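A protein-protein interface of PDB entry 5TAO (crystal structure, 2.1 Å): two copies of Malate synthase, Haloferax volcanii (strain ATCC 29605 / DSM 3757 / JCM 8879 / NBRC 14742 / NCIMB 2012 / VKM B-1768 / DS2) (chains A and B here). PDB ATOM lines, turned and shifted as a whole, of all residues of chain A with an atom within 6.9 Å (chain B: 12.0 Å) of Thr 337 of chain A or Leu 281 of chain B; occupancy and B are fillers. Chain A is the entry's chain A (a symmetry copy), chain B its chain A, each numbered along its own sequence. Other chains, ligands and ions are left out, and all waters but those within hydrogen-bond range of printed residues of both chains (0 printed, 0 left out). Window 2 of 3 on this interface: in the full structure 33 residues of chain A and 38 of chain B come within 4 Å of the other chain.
The backbone NH (N) of Leu 280 of chain B lies within hydrogen-bond range of the backbone carbonyl oxygen (O) of Ser 338 of chain A.
The backbone NH (N) of Asp 282 of chain B is in hydrogen-bond range of the backbone carbonyl oxygen (O) of Leu 336 of chain A (3.1 Å).
The side-chain hydroxyl (OG1) of Thr 337 of chain A is in hydrogen-bond range of the backbone carbonyl oxygen (O) of Leu 333 of chain A, at 2.7 Å.
The backbone carbonyl oxygen (O) of Leu 334 of chain A lies within hydrogen-bond range of the side-chain hydroxyl (OG1) of Thr 337 of chain A (3.2 Å).
Among the printed residues, pairs that only touch across the chains: Thr 337 of chain A with Leu 280 of chain B (3.1 Å), Tyr 339 of chain A with Ser 278 of chain B (3.3 Å), Tyr 339 of chain A with Trp 279 of chain B (3.4 Å), Leu 336 of chain A with Leu 281 of chain B (3.5 Å), Ser 338 of chain A with Trp 279 of chain B (3.5 Å), Tyr 339 of chain A with Gly 277 of chain B (3.6 Å), Leu 336 of chain A with Leu 280 of chain B (3.8 Å) and Thr 337 of chain A with Leu 281 of chain B (3.9 Å).
Glu 332 of chain A touches none of the printed residues of chain B.
No residue of chain B comes within 4 Å of Leu 333 of chain A.
No residue of chain B comes within 4 Å of Gly 335 of chain A.
Of chain B, only Trp 279 (3.5 Å) and Leu 280 (2.7 Å) come within 4 Å of Ser 338 of chain A.
Of the printed residues of chain B, Tyr 339 of chain A touches Gly 277, Ser 278 and Trp 279.
Printed residues of chain A within 4 Å of Gly 277 of chain B: Tyr 339.
Of the printed residues of chain A, Ser 278 of chain B touches Tyr 339.
Printed residues of chain A within 4 Å of Trp 279 of chain B: Ser 338 (3.5 Å) and Tyr 339 (3.4 Å).
Leu 281 of chain B touches just these residues of chain A: Leu 336 (3.5 Å) and Thr 337 (3.9 Å).
The nearest residue of chain B that does not touch Thr 337 of chain A is Trp 279 of chain B (4.1 Å).
Of the 6 printed residues of chain B, 6 touch a printed residue of chain A.
Among the printed residues, 10 pairs touch across the chains.
No position is printed for both chains.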
ATOM      1  N   GLU A 332      -7.952  14.320   4.857  1.00  0.00           N
ATOM      2  CA  GLU A 332      -7.938  14.947   6.171  1.00  0.00           C
ATOM      3  C   GLU A 332      -6.526  14.927   6.796  1.00  0.00           C
ATOM      4  O   GLU A 332      -6.207  15.763   7.615  1.00  0.00           O
ATOM      5  CB  GLU A 332      -8.879  14.178   7.089  1.00  0.00           C
ATOM      6  CG  GLU A 332      -9.349  14.927   8.310  1.00  0.00           C
ATOM      7  CD  GLU A 332     -10.724  15.555   8.115  1.00  0.00           C
ATOM      8  OE1 GLU A 332     -10.794  16.802   8.074  1.00  0.00           O
ATOM      9  OE2 GLU A 332     -11.734  14.814   8.006  1.00  0.00           O
ATOM     10  N   LEU A 333      -5.712  13.940   6.429  1.00  0.00           N
ATOM     11  CA  LEU A 333      -4.329  13.801   6.906  1.00  0.00           C
ATOM     12  C   LEU A 333      -3.342  14.756   6.220  1.00  0.00           C
ATOM     13  O   LEU A 333      -2.345  15.170   6.813  1.00  0.00           O
ATOM     14  CB  LEU A 333      -3.821  12.369   6.697  1.00  0.00           C
ATOM     15  CG  LEU A 333      -3.865  11.414   7.886  1.00  0.00           C
ATOM     16  CD1 LEU A 333      -5.121  11.579   8.727  1.00  0.00           C
ATOM     17  CD2 LEU A 333      -3.703  10.002   7.339  1.00  0.00           C
ATOM     18  N   LEU A 334      -3.593  15.054   4.961  1.00  0.00           N
ATOM     19  CA  LEU A 334      -2.869  16.101   4.306  1.00  0.00           C
ATOM     20  C   LEU A 334      -3.155  17.415   5.046  1.00  0.00           C
ATOM     21  O   LEU A 334      -2.241  18.161   5.366  1.00  0.00           O
ATOM     22  CB  LEU A 334      -3.229  16.154   2.825  1.00  0.00           C
ATOM     23  CG  LEU A 334      -2.601  15.028   1.985  1.00  0.00           C
ATOM     24  CD1 LEU A 334      -2.757  15.272   0.467  1.00  0.00           C
ATOM     25  CD2 LEU A 334      -1.130  14.805   2.371  1.00  0.00           C
ATOM     26  N   GLY A 335      -4.414  17.643   5.383  1.00  0.00           N
ATOM     27  CA  GLY A 335      -4.785  18.779   6.197  1.00  0.00           C
ATOM     28  C   GLY A 335      -4.090  18.795   7.540  1.00  0.00           C
ATOM     29  O   GLY A 335      -3.692  19.865   8.017  1.00  0.00           O
ATOM     30  N   LEU A 336      -3.933  17.616   8.144  1.00  0.00           N
ATOM     31  CA  LEU A 336      -3.345  17.499   9.486  1.00  0.00           C
ATOM     32  C   LEU A 336      -1.827  17.417   9.563  1.00  0.00           C
ATOM     33  O   LEU A 336      -1.241  17.416  10.663  1.00  0.00           O
ATOM     34  CB  LEU A 336      -3.945  16.316  10.258  1.00  0.00           C
ATOM     35  CG  LEU A 336      -5.076  16.743  11.206  1.00  0.00           C
ATOM     36  CD1 LEU A 336      -6.346  16.989  10.403  1.00  0.00           C
ATOM     37  CD2 LEU A 336      -5.337  15.736  12.328  1.00  0.00           C
ATOM     38  N   THR A 337      -1.182  17.267   8.437  1.00  0.00           N
ATOM     39  CA  THR A 337       0.255  17.128   8.447  1.00  0.00           C
ATOM     40  C   THR A 337       0.940  18.375   7.897  1.00  0.00           C
ATOM     41  O   THR A 337       0.342  19.206   7.198  1.00  0.00           O
ATOM     42  CB  THR A 337       0.699  15.966   7.558  1.00  0.00           C
ATOM     43  OG1 THR A 337       0.090  16.094   6.274  1.00  0.00           O
ATOM     44  CG2 THR A 337       0.307  14.689   8.182  1.00  0.00           C
ATOM     45  N   SER A 338       2.218  18.465   8.191  1.00  0.00           N
ATOM     46  CA  SER A 338       3.050  19.400   7.501  1.00  0.00           C
ATOM     47  C   SER A 338       4.426  18.797   7.471  1.00  0.00           C
ATOM     48  O   SER A 338       4.749  17.960   8.307  1.00  0.00           O
ATOM     49  CB  SER A 338       2.990  20.773   8.183  1.00  0.00           C
ATOM     50  OG  SER A 338       3.073  20.664   9.583  1.00  0.00           O
ATOM     51  N   TYR A 339       5.214  19.206   6.490  1.00  0.00           N
ATOM     52  CA  TYR A 339       6.550  18.693   6.260  1.00  0.00           C
ATOM     53  C   TYR A 339       7.672  19.742   6.461  1.00  0.00           C
ATOM     54  O   TYR A 339       7.652  20.813   5.860  1.00  0.00           O
ATOM     55  CB  TYR A 339       6.641  18.221   4.827  1.00  0.00           C
ATOM     56  CG  TYR A 339       7.945  17.560   4.454  1.00  0.00           C
ATOM     57  CD1 TYR A 339       8.310  16.343   5.024  1.00  0.00           C
ATOM     58  CD2 TYR A 339       8.792  18.123   3.514  1.00  0.00           C
ATOM     59  CE1 TYR A 339       9.489  15.712   4.672  1.00  0.00           C
ATOM     60  CE2 TYR A 339       9.986  17.507   3.164  1.00  0.00           C
ATOM     61  CZ  TYR A 339      10.325  16.291   3.751  1.00  0.00           C
ATOM     62  OH  TYR A 339      11.523  15.657   3.450  1.00  0.00           O
ATOM     63  N   GLY B 277      14.630  15.439   6.431  1.00  0.00           N
ATOM     64  CA  GLY B 277      13.212  15.786   6.577  1.00  0.00           C
ATOM     65  C   GLY B 277      12.453  15.178   7.750  1.00  0.00           C
ATOM     66  O   GLY B 277      12.956  14.248   8.409  1.00  0.00           O
ATOM     67  N   SER B 278      11.261  15.741   8.017  1.00  0.00           N
ATOM     68  CA  SER B 278      10.339  15.311   9.096  1.00  0.00           C
ATOM     69  C   SER B 278       8.901  15.701   8.817  1.00  0.00           C
ATOM     70  O   SER B 278       8.655  16.752   8.262  1.00  0.00           O
ATOM     71  CB  SER B 278      10.719  15.925  10.430  1.00  0.00           C
ATOM     72  OG  SER B 278      12.071  15.648  10.724  1.00  0.00           O
ATOM     73  N   TRP B 279       7.955  14.850   9.211  1.00  0.00           N
ATOM     74  CA  TRP B 279       6.519  15.060   9.036  1.00  0.00           C
ATOM     75  C   TRP B 279       5.999  15.400  10.399  1.00  0.00           C
ATOM     76  O   TRP B 279       6.427  14.773  11.358  1.00  0.00           O
ATOM     77  CB  TRP B 279       5.838  13.780   8.517  1.00  0.00           C
ATOM     78  CG  TRP B 279       6.156  13.550   7.086  1.00  0.00           C
ATOM     79  CD1 TRP B 279       7.330  13.080   6.584  1.00  0.00           C
ATOM     80  CD2 TRP B 279       5.319  13.849   5.959  1.00  0.00           C
ATOM     81  NE1 TRP B 279       7.286  13.078   5.211  1.00  0.00           N
ATOM     82  CE2 TRP B 279       6.064  13.548   4.802  1.00  0.00           C
ATOM     83  CE3 TRP B 279       4.027  14.363   5.822  1.00  0.00           C
ATOM     84  CZ2 TRP B 279       5.551  13.701   3.518  1.00  0.00           C
ATOM     85  CZ3 TRP B 279       3.522  14.541   4.564  1.00  0.00           C
ATOM     86  CH2 TRP B 279       4.281  14.198   3.411  1.00  0.00           C
ATOM     87  N   LEU B 280       5.118  16.405  10.506  1.00  0.00           N
ATOM     88  CA  LEU B 280       4.482  16.764  11.772  1.00  0.00           C
ATOM     89  C   LEU B 280       3.005  16.448  11.663  1.00  0.00           C
ATOM     90  O   LEU B 280       2.450  16.563  10.585  1.00  0.00           O
ATOM     91  CB  LEU B 280       4.657  18.263  12.084  1.00  0.00           C
ATOM     92  CG  LEU B 280       6.085  18.798  12.040  1.00  0.00           C
ATOM     93  CD1 LEU B 280       6.119  20.292  12.372  1.00  0.00           C
ATOM     94  CD2 LEU B 280       6.941  18.003  13.000  1.00  0.00           C
ATOM     95  N   LEU B 281       2.373  16.101  12.784  1.00  0.00           N
ATOM     96  CA  LEU B 281       0.937  15.843  12.828  1.00  0.00           C
ATOM     97  C   LEU B 281       0.213  16.567  13.986  1.00  0.00           C
ATOM     98  O   LEU B 281       0.759  16.665  15.083  1.00  0.00           O
ATOM     99  CB  LEU B 281       0.738  14.325  13.006  1.00  0.00           C
ATOM    100  CG  LEU B 281      -0.681  13.742  13.052  1.00  0.00           C
ATOM    101  CD1 LEU B 281      -1.239  13.609  11.648  1.00  0.00           C
ATOM    102  CD2 LEU B 281      -0.682  12.394  13.755  1.00  0.00           C
ATOM    103  N   ASP B 282      -1.030  17.008  13.764  1.00  0.00           N
ATOM    104  CA  ASP B 282      -1.983  17.233  14.891  1.00  0.00           C
ATOM    105  C   ASP B 282      -2.215  15.978  15.758  1.00  0.00           C
ATOM    106  O   ASP B 282      -3.092  15.945  16.635  1.00  0.00           O
ATOM    107  CB  ASP B 282      -3.336  17.721  14.366  1.00  0.00           C
ATOM    108  CG  ASP B 282      -3.464  19.242  14.373  1.00  0.00           C
ATOM    109  OD1 ASP B 282      -3.079  19.886  15.378  1.00  0.00           O
ATOM    110  OD2 ASP B 282      -3.988  19.789  13.383  1.00  0.00           O
